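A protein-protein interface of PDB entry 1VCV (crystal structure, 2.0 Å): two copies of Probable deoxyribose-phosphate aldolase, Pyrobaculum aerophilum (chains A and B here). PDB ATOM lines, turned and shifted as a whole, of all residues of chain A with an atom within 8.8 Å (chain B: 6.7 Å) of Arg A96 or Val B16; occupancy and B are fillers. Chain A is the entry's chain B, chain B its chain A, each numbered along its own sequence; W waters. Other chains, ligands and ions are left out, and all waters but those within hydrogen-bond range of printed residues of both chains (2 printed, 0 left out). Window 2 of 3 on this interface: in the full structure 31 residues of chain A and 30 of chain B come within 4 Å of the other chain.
Leu B14 touches Gly A90 (O to CA, 3.4 Å). Tyr B40 touches Gly A90 (OH to C, 3.5 Å). Leu A91 touches Tyr B40. CB of Lys A93 touches CG2 of Thr B15, 3.99 Å away. CB of Thr B15 touches OG of Ser A94, 3.1 Å away. Ser A94 touches Tyr B40 (OG to OH, 3.8 Å). Arg A96 touches Val B16 (NH2 to CG1, 3.4 Å).
Water W1 bridges OH of Tyr B40 (2.8 Å) and N of Leu A91 (3.4 Å). Water W2 lies within hydrogen-bond range of OD1 of Asp B17 (3.1 Å) and NH1 of Arg A96 (3.2 Å).
No position is printed for both chains.
The side-chain hydroxyl (OG) of Ser A94 is in hydrogen-bond range of the backbone NH (N) of Val B16 (3.0 Å).
Hydrophobic or aromatic side chains of chain A within 4 Å of the printed part of chain B: Leu A91. Of the 12 printed residues of chain B, 4 touch a printed residue of chain A. Printed residues of chain B that touch a printed residue of chain A: Leu B14, Thr B15, Val B16 and Tyr B40. Hydrophobic or aromatic side chains of chain B within 4 Å of the printed part of chain A: Val B16 and Tyr B40. Among the printed residues, no Asp or Glu carboxylate lies within 4 Å of a Lys or Arg side-chain nitrogen of the other chain.
The backbone carbonyl oxygen of Leu B14 sits at hydrogen-bond distance from the side-chain hydroxyl of Tyr B40 (2.6 Å). The backbone NH (N) of Thr B15 sits at hydrogen-bond distance from the side-chain carboxylate (OE2) of Glu B18, 3.0 Å away. The side-chain carboxylate (OE1) of Glu A129 lies within salt-bridge range of the side-chain amino group (NZ) of Lys A93, at 2.8 Å. The guanidinium group (NE) of Arg A96 is in salt-bridge range of the side-chain carboxylate (OE1) of Glu A99, at 3.5 Å. OG of Ser A94 lies within hydrogen-bond range of O of Gly A90 (2.8 Å). N of Val B16 lies within hydrogen-bond range of OH of Tyr B40, at 3.4 Å.
Of the printed residues of chain B, Leu A91 touches Tyr B40. Printed residues of chain B within 4 Å of Lys A93: Thr B15. Printed residues of chain B within 4 Å of Ser A94: Thr B15, Val B16 and Tyr B40. Arg A96 touches one residue of chain B. Of the printed residues of chain A, Val B16 touches Ser A94 (3.0 Å) and Arg A96 (3.4 Å). Of the printed residues of chain A, Tyr B40 touches Gly A90, Leu A91 and Ser A94. The nearest residue of chain B that does not touch Arg A96 is Asp B17 (4.4 Å). The nearest residue of chain A that does not touch Val B16 is Leu A91 (4.2 Å).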
ATOM      1  N   PRO A  88      22.548 -11.326 -14.656  1.00  0.00           N
ATOM      2  CA  PRO A  88      21.458 -10.341 -14.640  1.00  0.00           C
ATOM      3  C   PRO A  88      20.149 -11.023 -14.224  1.00  0.00           C
ATOM      4  O   PRO A  88      19.265 -11.257 -15.042  1.00  0.00           O
ATOM      5  CB  PRO A  88      21.432  -9.824 -16.078  1.00  0.00           C
ATOM      6  CG  PRO A  88      21.898 -11.008 -16.876  1.00  0.00           C
ATOM      7  CD  PRO A  88      23.042 -11.553 -16.029  1.00  0.00           C
ATOM      8  N   ILE A  89      20.045 -11.313 -12.930  1.00  0.00           N
ATOM      9  CA  ILE A  89      18.898 -12.008 -12.350  1.00  0.00           C
ATOM     10  C   ILE A  89      17.519 -11.589 -12.861  1.00  0.00           C
ATOM     11  O   ILE A  89      16.706 -12.438 -13.228  1.00  0.00           O
ATOM     12  CB  ILE A  89      18.917 -11.883 -10.814  1.00  0.00           C
ATOM     13  CG1 ILE A  89      20.254 -12.403 -10.275  1.00  0.00           C
ATOM     14  CG2 ILE A  89      17.763 -12.679 -10.214  1.00  0.00           C
ATOM     15  CD1 ILE A  89      20.429 -12.228  -8.783  1.00  0.00           C
ATOM     16  N   GLY A  90      17.256 -10.289 -12.883  1.00  0.00           N
ATOM     17  CA  GLY A  90      15.967  -9.811 -13.349  1.00  0.00           C
ATOM     18  C   GLY A  90      15.673 -10.242 -14.771  1.00  0.00           C
ATOM     19  O   GLY A  90      14.561 -10.659 -15.081  1.00  0.00           O
ATOM     20  N   LEU A  91      16.675 -10.135 -15.638  1.00  0.00           N
ATOM     21  CA  LEU A  91      16.523 -10.514 -17.036  1.00  0.00           C
ATOM     22  C   LEU A  91      16.344 -12.019 -17.194  1.00  0.00           C
ATOM     23  O   LEU A  91      15.648 -12.477 -18.098  1.00  0.00           O
ATOM     24  CB  LEU A  91      17.737 -10.032 -17.838  1.00  0.00           C
ATOM     25  CG  LEU A  91      17.947  -8.518 -17.740  1.00  0.00           C
ATOM     26  CD1 LEU A  91      19.052  -8.071 -18.700  1.00  0.00           C
ATOM     27  CD2 LEU A  91      16.637  -7.820 -18.077  1.00  0.00           C
ATOM     28  N   VAL A  92      16.981 -12.788 -16.319  1.00  0.00           N
ATOM     29  CA  VAL A  92      16.844 -14.240 -16.370  1.00  0.00           C
ATOM     30  C   VAL A  92      15.410 -14.605 -15.990  1.00  0.00           C
ATOM     31  O   VAL A  92      14.778 -15.435 -16.643  1.00  0.00           O
ATOM     32  CB  VAL A  92      17.810 -14.937 -15.392  1.00  0.00           C
ATOM     33  CG1 VAL A  92      17.471 -16.430 -15.295  1.00  0.00           C
ATOM     34  CG2 VAL A  92      19.241 -14.742 -15.856  1.00  0.00           C
ATOM     35  N   LYS A  93      14.897 -13.982 -14.934  1.00  0.00           N
ATOM     36  CA  LYS A  93      13.535 -14.259 -14.505  1.00  0.00           C
ATOM     37  C   LYS A  93      12.561 -13.826 -15.592  1.00  0.00           C
ATOM     38  O   LYS A  93      11.472 -14.387 -15.714  1.00  0.00           O
ATOM     39  CB  LYS A  93      13.224 -13.536 -13.193  1.00  0.00           C
ATOM     40  CG  LYS A  93      14.067 -14.012 -12.009  1.00  0.00           C
ATOM     41  CD  LYS A  93      13.999 -15.532 -11.835  1.00  0.00           C
ATOM     42  CE  LYS A  93      12.590 -16.020 -11.519  1.00  0.00           C
ATOM     43  NZ  LYS A  93      12.577 -17.472 -11.187  1.00  0.00           N
ATOM     44  N   SER A  94      12.963 -12.839 -16.392  1.00  0.00           N
ATOM     45  CA  SER A  94      12.127 -12.343 -17.481  1.00  0.00           C
ATOM     46  C   SER A  94      12.278 -13.211 -18.734  1.00  0.00           C
ATOM     47  O   SER A  94      11.580 -13.002 -19.727  1.00  0.00           O
ATOM     48  CB  SER A  94      12.502 -10.899 -17.824  1.00  0.00           C
ATOM     49  OG  SER A  94      12.378 -10.046 -16.697  1.00  0.00           O
ATOM     50  N   ARG A  95      13.189 -14.179 -18.677  1.00  0.00           N
ATOM     51  CA  ARG A  95      13.446 -15.074 -19.807  1.00  0.00           C
ATOM     52  C   ARG A  95      13.866 -14.267 -21.039  1.00  0.00           C
ATOM     53  O   ARG A  95      13.521 -14.611 -22.175  1.00  0.00           O
ATOM     54  CB  ARG A  95      12.196 -15.901 -20.137  1.00  0.00           C
ATOM     55  CG  ARG A  95      11.505 -16.534 -18.930  1.00  0.00           C
ATOM     56  CD  ARG A  95      12.398 -17.503 -18.182  1.00  0.00           C
ATOM     57  NE  ARG A  95      11.767 -17.967 -16.942  1.00  0.00           N
ATOM     58  CZ  ARG A  95      10.790 -18.870 -16.877  1.00  0.00           C
ATOM     59  NH1 ARG A  95      10.318 -19.430 -17.984  1.00  0.00           N
ATOM     60  NH2 ARG A  95      10.277 -19.209 -15.701  1.00  0.00           N
ATOM     61  N   ARG A  96      14.595 -13.179 -20.803  1.00  0.00           N
ATOM     62  CA  ARG A  96      15.080 -12.318 -21.880  1.00  0.00           C
ATOM     63  C   ARG A  96      16.470 -12.813 -22.275  1.00  0.00           C
ATOM     64  O   ARG A  96      17.479 -12.116 -22.115  1.00  0.00           O
ATOM     65  CB  ARG A  96      15.146 -10.869 -21.397  1.00  0.00           C
ATOM     66  CG  ARG A  96      13.797 -10.167 -21.308  1.00  0.00           C
ATOM     67  CD  ARG A  96      13.176 -10.014 -22.690  1.00  0.00           C
ATOM     68  NE  ARG A  96      12.330  -8.828 -22.805  1.00  0.00           N
ATOM     69  CZ  ARG A  96      11.195  -8.638 -22.140  1.00  0.00           C
ATOM     70  NH1 ARG A  96      10.747  -9.561 -21.294  1.00  0.00           N
ATOM     71  NH2 ARG A  96      10.504  -7.520 -22.323  1.00  0.00           N
ATOM     72  N   TRP A  97      16.506 -14.028 -22.807  1.00  0.00           N
ATOM     73  CA  TRP A  97      17.750 -14.669 -23.187  1.00  0.00           C
ATOM     74  C   TRP A  97      18.669 -13.887 -24.130  1.00  0.00           C
ATOM     75  O   TRP A  97      19.878 -13.862 -23.914  1.00  0.00           O
ATOM     76  CB  TRP A  97      17.431 -16.058 -23.743  1.00  0.00           C
ATOM     77  CG  TRP A  97      16.618 -16.872 -22.756  1.00  0.00           C
ATOM     78  CD1 TRP A  97      15.392 -17.434 -22.970  1.00  0.00           C
ATOM     79  CD2 TRP A  97      16.972 -17.194 -21.400  1.00  0.00           C
ATOM     80  NE1 TRP A  97      14.960 -18.084 -21.838  1.00  0.00           N
ATOM     81  CE2 TRP A  97      15.910 -17.955 -20.860  1.00  0.00           C
ATOM     82  CE3 TRP A  97      18.084 -16.915 -20.594  1.00  0.00           C
ATOM     83  CZ2 TRP A  97      15.925 -18.442 -19.544  1.00  0.00           C
ATOM     84  CZ3 TRP A  97      18.101 -17.400 -19.284  1.00  0.00           C
ATOM     85  CH2 TRP A  97      17.025 -18.156 -18.776  1.00  0.00           C
ATOM     86  N   ALA A  98      18.114 -13.245 -25.154  1.00  0.00           N
ATOM     87  CA  ALA A  98      18.934 -12.467 -26.092  1.00  0.00           C
ATOM     88  C   ALA A  98      19.712 -11.397 -25.324  1.00  0.00           C
ATOM     89  O   ALA A  98      20.911 -11.190 -25.558  1.00  0.00           O
ATOM     90  CB  ALA A  98      18.055 -11.813 -27.163  1.00  0.00           C
ATOM     91  N   GLU A  99      19.025 -10.732 -24.399  1.00  0.00           N
ATOM     92  CA  GLU A  99      19.641  -9.698 -23.577  1.00  0.00           C
ATOM     93  C   GLU A  99      20.603 -10.304 -22.557  1.00  0.00           C
ATOM     94  O   GLU A  99      21.671  -9.751 -22.296  1.00  0.00           O
ATOM     95  CB  GLU A  99      18.563  -8.891 -22.849  1.00  0.00           C
ATOM     96  CG  GLU A  99      17.564  -8.234 -23.779  1.00  0.00           C
ATOM     97  CD  GLU A  99      16.474  -7.486 -23.036  1.00  0.00           C
ATOM     98  OE1 GLU A  99      15.398  -7.266 -23.635  1.00  0.00           O
ATOM     99  OE2 GLU A  99      16.693  -7.114 -21.860  1.00  0.00           O
ATOM    100  N   VAL A 100      20.222 -11.437 -21.973  1.00  0.00           N
ATOM    101  CA  VAL A 100      21.078 -12.094 -20.993  1.00  0.00           C
ATOM    102  C   VAL A 100      22.412 -12.506 -21.615  1.00  0.00           C
ATOM    103  O   VAL A 100      23.469 -12.320 -21.009  1.00  0.00           O
ATOM    104  CB  VAL A 100      20.399 -13.342 -20.387  1.00  0.00           C
ATOM    105  CG1 VAL A 100      21.395 -14.101 -19.518  1.00  0.00           C
ATOM    106  CG2 VAL A 100      19.183 -12.924 -19.555  1.00  0.00           C
ATOM    107  N   ARG A 101      22.384 -13.066 -22.820  1.00  0.00           N
ATOM    108  CA  ARG A 101      23.642 -13.469 -23.423  1.00  0.00           C
ATOM    109  C   ARG A 101      24.465 -12.275 -23.888  1.00  0.00           C
ATOM    110  O   ARG A 101      25.681 -12.286 -23.743  1.00  0.00           O
ATOM    111  CB  ARG A 101      23.432 -14.473 -24.562  1.00  0.00           C
ATOM    112  CG  ARG A 101      22.382 -14.133 -25.583  1.00  0.00           C
ATOM    113  CD  ARG A 101      22.282 -15.291 -26.571  1.00  0.00           C
ATOM    114  NE  ARG A 101      22.021 -16.549 -25.876  1.00  0.00           N
ATOM    115  CZ  ARG A 101      22.311 -17.750 -26.362  1.00  0.00           C
ATOM    116  NH1 ARG A 101      22.880 -17.861 -27.552  1.00  0.00           N
ATOM    117  NH2 ARG A 101      22.036 -18.840 -25.656  1.00  0.00           N
ATOM    118  N   ARG A 102      23.816 -11.249 -24.430  1.00  0.00           N
ATOM    119  CA  ARG A 102      24.552 -10.058 -24.853  1.00  0.00           C
ATOM    120  C   ARG A 102      25.267  -9.475 -23.629  1.00  0.00           C
ATOM    121  O   ARG A 102      26.386  -8.969 -23.735  1.00  0.00           O
ATOM    122  CB  ARG A 102      23.609  -8.998 -25.447  1.00  0.00           C
ATOM    123  CG  ARG A 102      23.312  -9.163 -26.933  1.00  0.00           C
ATOM    124  CD  ARG A 102      22.648  -7.915 -27.508  1.00  0.00           C
ATOM    125  NE  ARG A 102      21.249  -7.793 -27.109  1.00  0.00           N
ATOM    126  CZ  ARG A 102      20.240  -8.397 -27.727  1.00  0.00           C
ATOM    127  NH1 ARG A 102      20.468  -9.170 -28.784  1.00  0.00           N
ATOM    128  NH2 ARG A 102      18.999  -8.225 -27.290  1.00  0.00           N
ATOM    129  N   ASP A 103      24.618  -9.552 -22.468  1.00  0.00           N
ATOM    130  CA  ASP A 103      25.199  -9.037 -21.231  1.00  0.00           C
ATOM    131  C   ASP A 103      26.353  -9.887 -20.693  1.00  0.00           C
ATOM    132  O   ASP A 103      27.441  -9.376 -20.445  1.00  0.00           O
ATOM    133  CB  ASP A 103      24.132  -8.929 -20.134  1.00  0.00           C
ATOM    134  CG  ASP A 103      24.720  -8.522 -18.788  1.00  0.00           C
ATOM    135  OD1 ASP A 103      24.808  -7.306 -18.508  1.00  0.00           O
ATOM    136  OD2 ASP A 103      25.110  -9.425 -18.013  1.00  0.00           O
ATOM    137  N   GLU A 129      14.998 -21.970 -16.299  1.00  0.00           N
ATOM    138  CA  GLU A 129      15.914 -20.841 -16.399  1.00  0.00           C
ATOM    139  C   GLU A 129      17.400 -21.193 -16.218  1.00  0.00           C
ATOM    140  O   GLU A 129      18.244 -20.709 -16.970  1.00  0.00           O
ATOM    141  CB  GLU A 129      15.542 -19.767 -15.364  1.00  0.00           C
ATOM    142  CG  GLU A 129      14.113 -19.235 -15.477  1.00  0.00           C
ATOM    143  CD  GLU A 129      13.626 -18.561 -14.197  1.00  0.00           C
ATOM    144  OE1 GLU A 129      14.009 -19.016 -13.095  1.00  0.00           O
ATOM    145  OE2 GLU A 129      12.842 -17.591 -14.289  1.00  0.00           O
ATOM    146  N   THR A 132      19.515 -22.950 -19.359  1.00  0.00           N
ATOM    147  CA  THR A 132      19.758 -22.024 -20.460  1.00  0.00           C
ATOM    148  C   THR A 132      20.791 -21.000 -19.965  1.00  0.00           C
ATOM    149  O   THR A 132      21.639 -20.545 -20.726  1.00  0.00           O
ATOM    150  CB  THR A 132      18.466 -21.293 -20.879  1.00  0.00           C
ATOM    151  OG1 THR A 132      17.486 -22.256 -21.281  1.00  0.00           O
ATOM    152  CG2 THR A 132      18.740 -20.336 -22.036  1.00  0.00           C
ATOM    153  N   LEU A 133      20.715 -20.643 -18.684  1.00  0.00           N
ATOM    154  CA  LEU A 133      21.673 -19.700 -18.108  1.00  0.00           C
ATOM    155  C   LEU A 133      23.074 -20.327 -18.124  1.00  0.00           C
ATOM    156  O   LEU A 133      24.060 -19.653 -18.429  1.00  0.00           O
ATOM    157  CB  LEU A 133      21.285 -19.339 -16.667  1.00  0.00           C
ATOM    158  CG  LEU A 133      22.182 -18.319 -15.948  1.00  0.00           C
ATOM    159  CD1 LEU A 133      22.298 -17.057 -16.789  1.00  0.00           C
ATOM    160  CD2 LEU A 133      21.604 -17.989 -14.583  1.00  0.00           C
ATOM    161  N   ILE A 136      24.594 -20.127 -21.496  1.00  0.00           N
ATOM    162  CA  ILE A 136      25.072 -18.775 -21.739  1.00  0.00           C
ATOM    163  C   ILE A 136      26.396 -18.509 -21.025  1.00  0.00           C
ATOM    164  O   ILE A 136      27.311 -17.918 -21.601  1.00  0.00           O
ATOM    165  CB  ILE A 136      24.004 -17.740 -21.304  1.00  0.00           C
ATOM    166  CG1 ILE A 136      22.752 -17.898 -22.178  1.00  0.00           C
ATOM    167  CG2 ILE A 136      24.561 -16.335 -21.416  1.00  0.00           C
ATOM    168  CD1 ILE A 136      21.571 -17.011 -21.763  1.00  0.00           C
ATOM    169  N   LEU B  14      12.898  -8.735  -9.934  1.00  0.00           N
ATOM    170  CA  LEU B  14      11.807  -8.008 -10.572  1.00  0.00           C
ATOM    171  C   LEU B  14      11.982  -8.197 -12.078  1.00  0.00           C
ATOM    172  O   LEU B  14      13.094  -8.086 -12.589  1.00  0.00           O
ATOM    173  CB  LEU B  14      11.886  -6.514 -10.234  1.00  0.00           C
ATOM    174  CG  LEU B  14      10.722  -5.674 -10.765  1.00  0.00           C
ATOM    175  CD1 LEU B  14       9.528  -5.869  -9.841  1.00  0.00           C
ATOM    176  CD2 LEU B  14      11.104  -4.190 -10.827  1.00  0.00           C
ATOM    177  N   THR B  15      10.895  -8.478 -12.790  1.00  0.00           N
ATOM    178  CA  THR B  15      10.980  -8.687 -14.235  1.00  0.00           C
ATOM    179  C   THR B  15      10.659  -7.422 -15.025  1.00  0.00           C
ATOM    180  O   THR B  15      10.129  -6.454 -14.480  1.00  0.00           O
ATOM    181  CB  THR B  15      10.004  -9.789 -14.705  1.00  0.00           C
ATOM    182  OG1 THR B  15       8.661  -9.318 -14.565  1.00  0.00           O
ATOM    183  CG2 THR B  15      10.169 -11.054 -13.863  1.00  0.00           C
ATOM    184  N   VAL B  16      10.985  -7.448 -16.317  1.00  0.00           N
ATOM    185  CA  VAL B  16      10.727  -6.320 -17.203  1.00  0.00           C
ATOM    186  C   VAL B  16       9.244  -5.955 -17.186  1.00  0.00           C
ATOM    187  O   VAL B  16       8.886  -4.783 -17.025  1.00  0.00           O
ATOM    188  CB  VAL B  16      11.153  -6.643 -18.659  1.00  0.00           C
ATOM    189  CG1 VAL B  16      10.655  -5.556 -19.604  1.00  0.00           C
ATOM    190  CG2 VAL B  16      12.671  -6.757 -18.743  1.00  0.00           C
ATOM    191  N   ASP B  17       8.386  -6.961 -17.345  1.00  0.00           N
ATOM    192  CA  ASP B  17       6.947  -6.737 -17.346  1.00  0.00           C
ATOM    193  C   ASP B  17       6.486  -6.092 -16.046  1.00  0.00           C
ATOM    194  O   ASP B  17       5.633  -5.199 -16.052  1.00  0.00           O
ATOM    195  CB  ASP B  17       6.202  -8.058 -17.564  1.00  0.00           C
ATOM    196  CG  ASP B  17       6.311  -8.556 -18.996  1.00  0.00           C
ATOM    197  OD1 ASP B  17       6.834  -7.805 -19.843  1.00  0.00           O
ATOM    198  OD2 ASP B  17       5.867  -9.690 -19.276  1.00  0.00           O
ATOM    199  N   GLU B  18       7.056  -6.544 -14.934  1.00  0.00           N
ATOM    200  CA  GLU B  18       6.719  -6.001 -13.627  1.00  0.00           C
ATOM    201  C   GLU B  18       7.220  -4.574 -13.497  1.00  0.00           C
ATOM    202  O   GLU B  18       6.535  -3.718 -12.938  1.00  0.00           O
ATOM    203  CB  GLU B  18       7.313  -6.880 -12.524  1.00  0.00           C
ATOM    204  CG  GLU B  18       6.508  -8.152 -12.295  1.00  0.00           C
ATOM    205  CD  GLU B  18       7.191  -9.124 -11.362  1.00  0.00           C
ATOM    206  OE1 GLU B  18       6.494 -10.012 -10.827  1.00  0.00           O
ATOM    207  OE2 GLU B  18       8.421  -9.010 -11.171  1.00  0.00           O
ATOM    208  N   ALA B  19       8.417  -4.319 -14.018  1.00  0.00           N
ATOM    209  CA  ALA B  19       8.997  -2.978 -13.973  1.00  0.00           C
ATOM    210  C   ALA B  19       8.156  -2.026 -14.827  1.00  0.00           C
ATOM    211  O   ALA B  19       7.924  -0.874 -14.451  1.00  0.00           O
ATOM    212  CB  ALA B  19      10.428  -3.010 -14.492  1.00  0.00           C
ATOM    213  N   VAL B  20       7.706  -2.514 -15.978  1.00  0.00           N
ATOM    214  CA  VAL B  20       6.896  -1.702 -16.875  1.00  0.00           C
ATOM    215  C   VAL B  20       5.550  -1.405 -16.238  1.00  0.00           C
ATOM    216  O   VAL B  20       5.072  -0.268 -16.282  1.00  0.00           O
ATOM    217  CB  VAL B  20       6.672  -2.406 -18.229  1.00  0.00           C
ATOM    218  CG1 VAL B  20       5.689  -1.606 -19.078  1.00  0.00           C
ATOM    219  CG2 VAL B  20       7.998  -2.547 -18.959  1.00  0.00           C
ATOM    220  N   ALA B  21       4.943  -2.433 -15.646  1.00  0.00           N
ATOM    221  CA  ALA B  21       3.656  -2.282 -14.984  1.00  0.00           C
ATOM    222  C   ALA B  21       3.781  -1.267 -13.840  1.00  0.00           C
ATOM    223  O   ALA B  21       2.883  -0.458 -13.609  1.00  0.00           O
ATOM    224  CB  ALA B  21       3.188  -3.625 -14.447  1.00  0.00           C
ATOM    225  N   GLY B  22       4.906  -1.312 -13.137  1.00  0.00           N
ATOM    226  CA  GLY B  22       5.125  -0.389 -12.040  1.00  0.00           C
ATOM    227  C   GLY B  22       5.124   1.061 -12.488  1.00  0.00           C
ATOM    228  O   GLY B  22       4.494   1.908 -11.850  1.00  0.00           O
ATOM    229  N   TYR B  40      16.676  -1.182 -15.550  1.00  0.00           N
ATOM    230  CA  TYR B  40      15.357  -0.916 -16.105  1.00  0.00           C
ATOM    231  C   TYR B  40      15.049   0.547 -16.403  1.00  0.00           C
ATOM    232  O   TYR B  40      13.932   0.874 -16.806  1.00  0.00           O
ATOM    233  CB  TYR B  40      14.277  -1.484 -15.170  1.00  0.00           C
ATOM    234  CG  TYR B  40      14.278  -2.998 -15.056  1.00  0.00           C
ATOM    235  CD1 TYR B  40      14.489  -3.799 -16.177  1.00  0.00           C
ATOM    236  CD2 TYR B  40      14.000  -3.630 -13.841  1.00  0.00           C
ATOM    237  CE1 TYR B  40      14.416  -5.192 -16.098  1.00  0.00           C
ATOM    238  CE2 TYR B  40      13.925  -5.028 -13.753  1.00  0.00           C
ATOM    239  CZ  TYR B  40      14.132  -5.801 -14.890  1.00  0.00           C
ATOM    240  OH  TYR B  40      14.043  -7.181 -14.830  1.00  0.00           O
ATOM    241  N   VAL B  43      13.879   1.195 -20.241  1.00  0.00           N
ATOM    242  CA  VAL B  43      12.560   0.683 -20.596  1.00  0.00           C
ATOM    243  C   VAL B  43      11.428   1.445 -19.905  1.00  0.00           C
ATOM    244  O   VAL B  43      10.340   1.600 -20.463  1.00  0.00           O
ATOM    245  CB  VAL B  43      12.435  -0.831 -20.278  1.00  0.00           C
ATOM    246  CG1 VAL B  43      12.378  -1.058 -18.779  1.00  0.00           C
ATOM    247  CG2 VAL B  43      11.208  -1.403 -20.965  1.00  0.00           C
ATOM    248  N   VAL B  44      11.694   1.926 -18.696  1.00  0.00           N
ATOM    249  CA  VAL B  44      10.703   2.678 -17.931  1.00  0.00           C
ATOM    250  C   VAL B  44      10.622   4.162 -18.321  1.00  0.00           C
ATOM    251  O   VAL B  44       9.554   4.771 -18.244  1.00  0.00           O
ATOM    252  CB  VAL B  44      11.003   2.561 -16.420  1.00  0.00           C
ATOM    253  CG1 VAL B  44      10.167   3.552 -15.639  1.00  0.00           C
ATOM    254  CG2 VAL B  44      10.717   1.136 -15.957  1.00  0.00           C
HETATM  255  O   HOH W   1      16.744  -7.060 -14.247  1.00  0.00           O
HETATM  256  O   HOH W   2       7.675  -9.553 -22.319  1.00  0.00           O
